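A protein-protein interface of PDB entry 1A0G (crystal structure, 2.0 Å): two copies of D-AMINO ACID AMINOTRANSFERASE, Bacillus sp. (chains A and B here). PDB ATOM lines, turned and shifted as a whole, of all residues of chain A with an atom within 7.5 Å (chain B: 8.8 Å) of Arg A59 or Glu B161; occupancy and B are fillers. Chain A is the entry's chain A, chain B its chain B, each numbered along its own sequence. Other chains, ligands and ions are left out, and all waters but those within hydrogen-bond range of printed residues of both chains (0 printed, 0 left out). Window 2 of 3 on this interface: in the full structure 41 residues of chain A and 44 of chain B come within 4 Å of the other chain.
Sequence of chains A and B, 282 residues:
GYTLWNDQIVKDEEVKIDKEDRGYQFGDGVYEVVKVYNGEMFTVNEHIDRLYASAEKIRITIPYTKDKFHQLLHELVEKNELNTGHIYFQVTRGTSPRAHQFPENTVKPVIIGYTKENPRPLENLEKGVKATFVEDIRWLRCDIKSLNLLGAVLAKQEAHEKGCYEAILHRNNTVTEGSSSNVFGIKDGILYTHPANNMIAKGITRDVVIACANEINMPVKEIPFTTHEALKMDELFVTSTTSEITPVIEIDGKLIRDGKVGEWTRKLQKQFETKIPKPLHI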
ATOM      1  N   ASP A  28      17.811   6.406 -17.007  1.00  0.00           N
ATOM      2  CA  ASP A  28      17.960   7.506 -16.061  1.00  0.00           C
ATOM      3  C   ASP A  28      18.883   8.643 -16.499  1.00  0.00           C
ATOM      4  O   ASP A  28      19.996   8.822 -15.970  1.00  0.00           O
ATOM      5  CB  ASP A  28      18.391   6.935 -14.709  1.00  0.00           C
ATOM      6  CG  ASP A  28      18.307   7.938 -13.585  1.00  0.00           C
ATOM      7  OD1 ASP A  28      17.881   9.100 -13.797  1.00  0.00           O
ATOM      8  OD2 ASP A  28      18.652   7.544 -12.453  1.00  0.00           O
ATOM      9  N   ALA A  53      17.355  22.207 -17.215  1.00  0.00           N
ATOM     10  CA  ALA A  53      16.014  22.179 -16.642  1.00  0.00           C
ATOM     11  C   ALA A  53      15.540  20.729 -16.552  1.00  0.00           C
ATOM     12  O   ALA A  53      14.953  20.333 -15.555  1.00  0.00           O
ATOM     13  CB  ALA A  53      15.039  23.003 -17.496  1.00  0.00           C
ATOM     14  N   SER A  54      15.776  19.951 -17.603  1.00  0.00           N
ATOM     15  CA  SER A  54      15.386  18.547 -17.634  1.00  0.00           C
ATOM     16  C   SER A  54      16.127  17.787 -16.530  1.00  0.00           C
ATOM     17  O   SER A  54      15.536  17.002 -15.793  1.00  0.00           O
ATOM     18  CB  SER A  54      15.714  17.925 -18.990  1.00  0.00           C
ATOM     19  OG  SER A  54      14.846  18.370 -20.013  1.00  0.00           O
ATOM     20  N   ALA A  55      17.423  18.040 -16.404  1.00  0.00           N
ATOM     21  CA  ALA A  55      18.219  17.370 -15.378  1.00  0.00           C
ATOM     22  C   ALA A  55      17.700  17.730 -13.987  1.00  0.00           C
ATOM     23  O   ALA A  55      17.493  16.856 -13.145  1.00  0.00           O
ATOM     24  CB  ALA A  55      19.682  17.734 -15.521  1.00  0.00           C
ATOM     25  N   GLU A  56      17.407  19.005 -13.782  1.00  0.00           N
ATOM     26  CA  GLU A  56      16.911  19.478 -12.502  1.00  0.00           C
ATOM     27  C   GLU A  56      15.589  18.824 -12.136  1.00  0.00           C
ATOM     28  O   GLU A  56      15.366  18.481 -10.973  1.00  0.00           O
ATOM     29  CB  GLU A  56      16.760  20.989 -12.542  1.00  0.00           C
ATOM     30  CG  GLU A  56      16.706  21.687 -11.186  1.00  0.00           C
ATOM     31  CD  GLU A  56      16.710  23.206 -11.325  1.00  0.00           C
ATOM     32  OE1 GLU A  56      16.970  23.693 -12.459  1.00  0.00           O
ATOM     33  OE2 GLU A  56      16.456  23.920 -10.314  1.00  0.00           O
ATOM     34  N   LYS A  57      14.737  18.582 -13.129  1.00  0.00           N
ATOM     35  CA  LYS A  57      13.441  17.958 -12.866  1.00  0.00           C
ATOM     36  C   LYS A  57      13.538  16.536 -12.302  1.00  0.00           C
ATOM     37  O   LYS A  57      12.623  16.086 -11.617  1.00  0.00           O
ATOM     38  CB  LYS A  57      12.555  17.983 -14.116  1.00  0.00           C
ATOM     39  CG  LYS A  57      11.987  19.356 -14.443  1.00  0.00           C
ATOM     40  CD  LYS A  57      11.436  19.392 -15.867  1.00  0.00           C
ATOM     41  CE  LYS A  57      10.729  20.703 -16.175  1.00  0.00           C
ATOM     42  NZ  LYS A  57      10.367  20.764 -17.619  1.00  0.00           N
ATOM     43  N   ILE A  58      14.610  15.813 -12.628  1.00  0.00           N
ATOM     44  CA  ILE A  58      14.793  14.464 -12.104  1.00  0.00           C
ATOM     45  C   ILE A  58      15.978  14.426 -11.137  1.00  0.00           C
ATOM     46  O   ILE A  58      16.519  13.364 -10.801  1.00  0.00           O
ATOM     47  CB  ILE A  58      14.925  13.405 -13.207  1.00  0.00           C
ATOM     48  CG1 ILE A  58      16.140  13.674 -14.101  1.00  0.00           C
ATOM     49  CG2 ILE A  58      13.633  13.323 -14.011  1.00  0.00           C
ATOM     50  CD1 ILE A  58      16.442  12.491 -15.021  1.00  0.00           C
ATOM     51  N   ARG A  59      16.353  15.620 -10.694  1.00  0.00           N
ATOM     52  CA  ARG A  59      17.414  15.870  -9.733  1.00  0.00           C
ATOM     53  C   ARG A  59      18.835  15.393 -10.026  1.00  0.00           C
ATOM     54  O   ARG A  59      19.535  14.871  -9.149  1.00  0.00           O
ATOM     55  CB  ARG A  59      16.943  15.467  -8.339  1.00  0.00           C
ATOM     56  CG  ARG A  59      15.662  16.222  -7.959  1.00  0.00           C
ATOM     57  CD  ARG A  59      14.747  15.421  -7.052  1.00  0.00           C
ATOM     58  NE  ARG A  59      15.336  15.318  -5.728  1.00  0.00           N
ATOM     59  CZ  ARG A  59      14.957  14.459  -4.787  1.00  0.00           C
ATOM     60  NH1 ARG A  59      13.962  13.596  -5.000  1.00  0.00           N
ATOM     61  NH2 ARG A  59      15.599  14.462  -3.628  1.00  0.00           N
ATOM     62  N   ILE A  60      19.268  15.607 -11.259  1.00  0.00           N
ATOM     63  CA  ILE A  60      20.613  15.266 -11.655  1.00  0.00           C
ATOM     64  C   ILE A  60      21.324  16.608 -11.588  1.00  0.00           C
ATOM     65  O   ILE A  60      20.821  17.596 -12.124  1.00  0.00           O
ATOM     66  CB  ILE A  60      20.669  14.725 -13.110  1.00  0.00           C
ATOM     67  CG1 ILE A  60      20.177  13.280 -13.172  1.00  0.00           C
ATOM     68  CG2 ILE A  60      22.076  14.838 -13.670  1.00  0.00           C
ATOM     69  CD1 ILE A  60      20.312  12.627 -14.542  1.00  0.00           C
ATOM     70  N   THR A  61      22.435  16.685 -10.862  1.00  0.00           N
ATOM     71  CA  THR A  61      23.186  17.946 -10.786  1.00  0.00           C
ATOM     72  C   THR A  61      24.354  17.881 -11.755  1.00  0.00           C
ATOM     73  O   THR A  61      25.277  17.101 -11.562  1.00  0.00           O
ATOM     74  CB  THR A  61      23.747  18.221  -9.380  1.00  0.00           C
ATOM     75  OG1 THR A  61      22.677  18.236  -8.430  1.00  0.00           O
ATOM     76  CG2 THR A  61      24.441  19.574  -9.356  1.00  0.00           C
ATOM     77  N   ILE A  62      24.309  18.688 -12.806  1.00  0.00           N
ATOM     78  CA  ILE A  62      25.381  18.681 -13.791  1.00  0.00           C
ATOM     79  C   ILE A  62      26.598  19.380 -13.199  1.00  0.00           C
ATOM     80  O   ILE A  62      26.524  20.541 -12.816  1.00  0.00           O
ATOM     81  CB  ILE A  62      24.896  19.288 -15.117  1.00  0.00           C
ATOM     82  CG1 ILE A  62      23.734  18.428 -15.638  1.00  0.00           C
ATOM     83  CG2 ILE A  62      26.013  19.294 -16.144  1.00  0.00           C
ATOM     84  CD1 ILE A  62      22.983  18.989 -16.819  1.00  0.00           C
ATOM     85  N   ARG A  93      22.620   9.870 -14.603  1.00  0.00           N
ATOM     86  CA  ARG A  93      22.924  10.063 -13.189  1.00  0.00           C
ATOM     87  C   ARG A  93      24.286   9.464 -12.790  1.00  0.00           C
ATOM     88  O   ARG A  93      24.865   9.844 -11.771  1.00  0.00           O
ATOM     89  CB  ARG A  93      21.793   9.494 -12.317  1.00  0.00           C
ATOM     90  CG  ARG A  93      21.777  10.020 -10.872  1.00  0.00           C
ATOM     91  CD  ARG A  93      20.586   9.463 -10.062  1.00  0.00           C
ATOM     92  NE  ARG A  93      19.336   9.705 -10.764  1.00  0.00           N
ATOM     93  CZ  ARG A  93      18.665  10.852 -10.742  1.00  0.00           C
ATOM     94  NH1 ARG A  93      19.096  11.875 -10.025  1.00  0.00           N
ATOM     95  NH2 ARG A  93      17.588  10.987 -11.494  1.00  0.00           N
ATOM     96  N   GLN A 101      16.574   3.568  -6.203  1.00  0.00           N
ATOM     97  CA  GLN A 101      16.773   4.871  -5.590  1.00  0.00           C
ATOM     98  C   GLN A 101      18.114   5.501  -5.976  1.00  0.00           C
ATOM     99  O   GLN A 101      19.042   4.811  -6.409  1.00  0.00           O
ATOM    100  CB  GLN A 101      16.639   4.785  -4.069  1.00  0.00           C
ATOM    101  CG  GLN A 101      17.825   4.176  -3.332  1.00  0.00           C
ATOM    102  CD  GLN A 101      17.833   2.660  -3.339  1.00  0.00           C
ATOM    103  OE1 GLN A 101      16.973   1.996  -3.945  1.00  0.00           O
ATOM    104  NE2 GLN A 101      18.796   2.096  -2.634  1.00  0.00           N
ATOM    105  N   PHE A 102      18.221   6.810  -5.794  1.00  0.00           N
ATOM    106  CA  PHE A 102      19.440   7.537  -6.143  1.00  0.00           C
ATOM    107  C   PHE A 102      20.675   7.003  -5.424  1.00  0.00           C
ATOM    108  O   PHE A 102      20.575   6.503  -4.304  1.00  0.00           O
ATOM    109  CB  PHE A 102      19.301   9.035  -5.811  1.00  0.00           C
ATOM    110  CG  PHE A 102      18.197   9.743  -6.568  1.00  0.00           C
ATOM    111  CD1 PHE A 102      17.440   9.079  -7.525  1.00  0.00           C
ATOM    112  CD2 PHE A 102      17.920  11.085  -6.305  1.00  0.00           C
ATOM    113  CE1 PHE A 102      16.403   9.733  -8.200  1.00  0.00           C
ATOM    114  CE2 PHE A 102      16.886  11.747  -6.977  1.00  0.00           C
ATOM    115  CZ  PHE A 102      16.134  11.064  -7.931  1.00  0.00           C
ATOM    116  N   ASN A 105      25.377  10.751  -3.323  1.00  0.00           N
ATOM    117  CA  ASN A 105      25.640  12.013  -4.038  1.00  0.00           C
ATOM    118  C   ASN A 105      27.078  12.214  -4.506  1.00  0.00           C
ATOM    119  O   ASN A 105      27.406  13.198  -5.130  1.00  0.00           O
ATOM    120  CB  ASN A 105      25.232  13.209  -3.190  1.00  0.00           C
ATOM    121  CG  ASN A 105      23.727  13.294  -2.973  1.00  0.00           C
ATOM    122  OD1 ASN A 105      23.249  13.284  -1.830  1.00  0.00           O
ATOM    123  ND2 ASN A 105      22.973  13.358  -4.060  1.00  0.00           N
ATOM    124  N   LYS B 130       7.471  -0.283   6.328  1.00  0.00           N
ATOM    125  CA  LYS B 130       6.581   0.872   6.158  1.00  0.00           C
ATOM    126  C   LYS B 130       6.544   1.199   4.659  1.00  0.00           C
ATOM    127  O   LYS B 130       7.548   1.036   3.962  1.00  0.00           O
ATOM    128  CB  LYS B 130       7.131   2.109   6.884  1.00  0.00           C
ATOM    129  CG  LYS B 130       7.355   1.945   8.369  1.00  0.00           C
ATOM    130  CD  LYS B 130       7.934   3.216   8.976  1.00  0.00           C
ATOM    131  CE  LYS B 130       9.390   3.425   8.622  1.00  0.00           C
ATOM    132  NZ  LYS B 130       9.866   4.771   9.074  1.00  0.00           N
ATOM    133  N   THR B 132       4.654   3.935   1.421  1.00  0.00           N
ATOM    134  CA  THR B 132       4.051   5.224   1.145  1.00  0.00           C
ATOM    135  C   THR B 132       3.334   5.146  -0.190  1.00  0.00           C
ATOM    136  O   THR B 132       3.655   4.303  -1.016  1.00  0.00           O
ATOM    137  CB  THR B 132       5.098   6.333   1.116  1.00  0.00           C
ATOM    138  OG1 THR B 132       4.445   7.596   1.026  1.00  0.00           O
ATOM    139  CG2 THR B 132       6.046   6.164  -0.059  1.00  0.00           C
ATOM    140  N   LEU B 150      12.222   5.065 -15.310  1.00  0.00           N
ATOM    141  CA  LEU B 150      12.379   6.357 -14.662  1.00  0.00           C
ATOM    142  C   LEU B 150      11.253   6.683 -13.667  1.00  0.00           C
ATOM    143  O   LEU B 150      11.510   7.246 -12.610  1.00  0.00           O
ATOM    144  CB  LEU B 150      12.592   7.452 -15.705  1.00  0.00           C
ATOM    145  CG  LEU B 150      13.110   8.785 -15.193  1.00  0.00           C
ATOM    146  CD1 LEU B 150      14.360   8.598 -14.346  1.00  0.00           C
ATOM    147  CD2 LEU B 150      13.388   9.664 -16.374  1.00  0.00           C
ATOM    148  N   VAL B 153      12.068   4.797 -10.565  1.00  0.00           N
ATOM    149  CA  VAL B 153      13.211   5.384  -9.916  1.00  0.00           C
ATOM    150  C   VAL B 153      12.733   6.551  -9.057  1.00  0.00           C
ATOM    151  O   VAL B 153      13.083   6.648  -7.879  1.00  0.00           O
ATOM    152  CB  VAL B 153      14.233   5.870 -10.959  1.00  0.00           C
ATOM    153  CG1 VAL B 153      15.206   6.891 -10.346  1.00  0.00           C
ATOM    154  CG2 VAL B 153      14.989   4.696 -11.506  1.00  0.00           C
ATOM    155  N   LEU B 154      11.906   7.420  -9.636  1.00  0.00           N
ATOM    156  CA  LEU B 154      11.416   8.581  -8.908  1.00  0.00           C
ATOM    157  C   LEU B 154      10.549   8.182  -7.713  1.00  0.00           C
ATOM    158  O   LEU B 154      10.676   8.758  -6.639  1.00  0.00           O
ATOM    159  CB  LEU B 154      10.670   9.518  -9.855  1.00  0.00           C
ATOM    160  CG  LEU B 154      11.538  10.195 -10.920  1.00  0.00           C
ATOM    161  CD1 LEU B 154      10.645  10.969 -11.868  1.00  0.00           C
ATOM    162  CD2 LEU B 154      12.553  11.136 -10.276  1.00  0.00           C
ATOM    163  N   ALA B 155       9.736   7.142  -7.900  1.00  0.00           N
ATOM    164  CA  ALA B 155       8.849   6.614  -6.870  1.00  0.00           C
ATOM    165  C   ALA B 155       9.620   6.015  -5.694  1.00  0.00           C
ATOM    166  O   ALA B 155       9.345   6.338  -4.534  1.00  0.00           O
ATOM    167  CB  ALA B 155       7.923   5.580  -7.470  1.00  0.00           C
ATOM    168  N   LYS B 156      10.578   5.140  -5.994  1.00  0.00           N
ATOM    169  CA  LYS B 156      11.405   4.502  -4.968  1.00  0.00           C
ATOM    170  C   LYS B 156      12.203   5.564  -4.194  1.00  0.00           C
ATOM    171  O   LYS B 156      12.361   5.468  -2.976  1.00  0.00           O
ATOM    172  CB  LYS B 156      12.360   3.491  -5.623  1.00  0.00           C
ATOM    173  CG  LYS B 156      13.280   2.746  -4.661  1.00  0.00           C
ATOM    174  CD  LYS B 156      12.586   1.562  -4.004  1.00  0.00           C
ATOM    175  CE  LYS B 156      12.244   0.520  -5.039  1.00  0.00           C
ATOM    176  NZ  LYS B 156      11.604  -0.657  -4.415  1.00  0.00           N
ATOM    177  N   GLN B 157      12.699   6.578  -4.895  1.00  0.00           N
ATOM    178  CA  GLN B 157      13.473   7.624  -4.232  1.00  0.00           C
ATOM    179  C   GLN B 157      12.599   8.368  -3.247  1.00  0.00           C
ATOM    180  O   GLN B 157      13.053   8.752  -2.166  1.00  0.00           O
ATOM    181  CB  GLN B 157      14.057   8.608  -5.249  1.00  0.00           C
ATOM    182  CG  GLN B 157      14.890   9.742  -4.630  1.00  0.00           C
ATOM    183  CD  GLN B 157      16.057   9.224  -3.797  1.00  0.00           C
ATOM    184  OE1 GLN B 157      16.471   8.069  -3.927  1.00  0.00           O
ATOM    185  NE2 GLN B 157      16.599  10.079  -2.948  1.00  0.00           N
ATOM    186  N   GLU B 158      11.346   8.583  -3.632  1.00  0.00           N
ATOM    187  CA  GLU B 158      10.396   9.292  -2.786  1.00  0.00           C
ATOM    188  C   GLU B 158      10.148   8.480  -1.511  1.00  0.00           C
ATOM    189  O   GLU B 158      10.165   9.033  -0.405  1.00  0.00           O
ATOM    190  CB  GLU B 158       9.078   9.533  -3.537  1.00  0.00           C
ATOM    191  CG  GLU B 158       8.264  10.687  -2.958  1.00  0.00           C
ATOM    192  CD  GLU B 158       6.896  10.861  -3.600  1.00  0.00           C
ATOM    193  OE1 GLU B 158       6.829  11.078  -4.829  1.00  0.00           O
ATOM    194  OE2 GLU B 158       5.892  10.786  -2.859  1.00  0.00           O
ATOM    195  N   ALA B 159       9.956   7.170  -1.661  1.00  0.00           N
ATOM    196  CA  ALA B 159       9.723   6.299  -0.503  1.00  0.00           C
ATOM    197  C   ALA B 159      10.939   6.306   0.417  1.00  0.00           C
ATOM    198  O   ALA B 159      10.826   6.537   1.615  1.00  0.00           O
ATOM    199  CB  ALA B 159       9.412   4.895  -0.951  1.00  0.00           C
ATOM    200  N   HIS B 160      12.112   6.108  -0.174  1.00  0.00           N
ATOM    201  CA  HIS B 160      13.381   6.096   0.542  1.00  0.00           C
ATOM    202  C   HIS B 160      13.628   7.363   1.379  1.00  0.00           C
ATOM    203  O   HIS B 160      14.142   7.275   2.495  1.00  0.00           O
ATOM    204  CB  HIS B 160      14.514   5.908  -0.473  1.00  0.00           C
ATOM    205  CG  HIS B 160      15.864   5.695   0.142  1.00  0.00           C
ATOM    206  ND1 HIS B 160      16.468   4.455   0.211  1.00  0.00           N
ATOM    207  CD2 HIS B 160      16.744   6.572   0.685  1.00  0.00           C
ATOM    208  CE1 HIS B 160      17.660   4.580   0.765  1.00  0.00           C
ATOM    209  NE2 HIS B 160      17.851   5.856   1.063  1.00  0.00           N
ATOM    210  N   GLU B 161      13.295   8.534   0.836  1.00  0.00           N
ATOM    211  CA  GLU B 161      13.499   9.807   1.536  1.00  0.00           C
ATOM    212  C   GLU B 161      12.614   9.975   2.757  1.00  0.00           C
ATOM    213  O   GLU B 161      12.954  10.718   3.673  1.00  0.00           O
ATOM    214  CB  GLU B 161      13.278  10.995   0.601  1.00  0.00           C
ATOM    215  CG  GLU B 161      14.210  11.021  -0.572  1.00  0.00           C
ATOM    216  CD  GLU B 161      14.096  12.287  -1.385  1.00  0.00           C
ATOM    217  OE1 GLU B 161      13.084  12.459  -2.102  1.00  0.00           O
ATOM    218  OE2 GLU B 161      15.033  13.108  -1.305  1.00  0.00           O
ATOM    219  N   LYS B 162      11.464   9.310   2.752  1.00  0.00           N
ATOM    220  CA  LYS B 162      10.531   9.369   3.873  1.00  0.00           C
ATOM    221  C   LYS B 162      10.771   8.218   4.867  1.00  0.00           C
ATOM    222  O   LYS B 162      10.023   8.047   5.837  1.00  0.00           O
ATOM    223  CB  LYS B 162       9.087   9.378   3.343  1.00  0.00           C
ATOM    224  CG  LYS B 162       8.636  10.776   2.934  1.00  0.00           C
ATOM    225  CD  LYS B 162       7.843  10.816   1.636  1.00  0.00           C
ATOM    226  CE  LYS B 162       6.454  10.235   1.772  1.00  0.00           C
ATOM    227  NZ  LYS B 162       5.631  10.577   0.574  1.00  0.00           N
ATOM    228  N   GLY B 163      11.843   7.461   4.634  1.00  0.00           N
ATOM    229  CA  GLY B 163      12.199   6.351   5.498  1.00  0.00           C
ATOM    230  C   GLY B 163      11.393   5.094   5.239  1.00  0.00           C
ATOM    231  O   GLY B 163      11.379   4.196   6.065  1.00  0.00           O
ATOM    232  N   CYS B 164      10.750   5.015   4.079  1.00  0.00           N
ATOM    233  CA  CYS B 164       9.930   3.863   3.727  1.00  0.00           C
ATOM    234  C   CYS B 164      10.693   2.908   2.844  1.00  0.00           C
ATOM    235  O   CYS B 164      11.671   3.301   2.215  1.00  0.00           O
ATOM    236  CB  CYS B 164       8.643   4.333   3.047  1.00  0.00           C
ATOM    237  SG  CYS B 164       7.715   5.456   4.087  1.00  0.00           S
ATOM    238  N   TYR B 165      10.197   1.680   2.733  1.00  0.00           N
ATOM    239  CA  TYR B 165      10.858   0.652   1.944  1.00  0.00           C
ATOM    240  C   TYR B 165      10.378   0.568   0.506  1.00  0.00           C
ATOM    241  O   TYR B 165      11.158   0.296  -0.406  1.00  0.00           O
ATOM    242  CB  TYR B 165      10.696  -0.720   2.634  1.00  0.00           C
ATOM    243  CG  TYR B 165      11.185  -1.917   1.834  1.00  0.00           C
ATOM    244  CD1 TYR B 165      12.549  -2.215   1.732  1.00  0.00           C
ATOM    245  CD2 TYR B 165      10.281  -2.746   1.173  1.00  0.00           C
ATOM    246  CE1 TYR B 165      12.990  -3.298   0.985  1.00  0.00           C
ATOM    247  CE2 TYR B 165      10.712  -3.826   0.432  1.00  0.00           C
ATOM    248  CZ  TYR B 165      12.063  -4.095   0.342  1.00  0.00           C
ATOM    249  OH  TYR B 165      12.478  -5.162  -0.413  1.00  0.00           O
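The guanidinium group of Arg A59 is in salt-bridge range of the side-chain carboxylate of Glu B161, 2.7 Å away. The backbone NH (N) of Phe A102 is in hydrogen-bond range of the side-chain amide oxygen (OE1) of Gln B157 (2.9 Å).
The guanidinium group (NE) of Arg A93 is in salt-bridge range of the side-chain carboxylate (OD2) of Asp A28 (2.8 Å). NH1 of Arg A93 is in hydrogen-bond range of O of Arg A59, 3.2 Å away.
Among the printed residues, pairs that only touch across the chains: Asp A28 with Leu B150 (3.6 Å), Arg A59 with Gln B157 (3.98 Å), Gln A101 with Lys B156 (3.7 Å), Gln A101 with Gln B157 (3.3 Å), Gln A101 with His B160 (3.8 Å) and Phe A102 with Val B153 (3.8 Å).
Of the printed residues of chain B, Arg A59 touches Gln B157 (3.98 Å) and Glu B161 (2.7 Å). Printed residues of chain A within 4 Å of Glu B161: Arg A59. Printed residues of chain B within 4 Å of Gln A101: Lys B156 (3.7 Å), Gln B157 (3.3 Å) and His B160 (3.8 Å). Printed residues of chain A within 4 Å of Val B153: Phe A102. Of the printed residues of chain A, His B160 touches Gln A101 (3.8 Å). Printed residues of chain B within 4 Å of Phe A102: Val B153 (3.8 Å) and Gln B157 (2.9 Å). Arg A93 touches none of the printed residues of chain B. The nearest printed residue of chain B that does not touch Arg A59 is Leu B154 (5.8 Å).
Hydrophobic or aromatic side chains of chain B within 4 Å of the printed part of chain A: Leu B150, Val B153 and His B160. Hydrophobic or aromatic side chains of chain A within 4 Å of the printed part of chain B: Phe A102. Among the printed residues, Asp or Glu carboxylates within 4 Å of a Lys or Arg side-chain nitrogen of the other chain: Arg A59 with Glu B161 (2.7 Å).
No position is printed for both chains. Of the 8 pairs that touch across the chains among the printed residues, none has its exchanged pair printed and touching as well.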
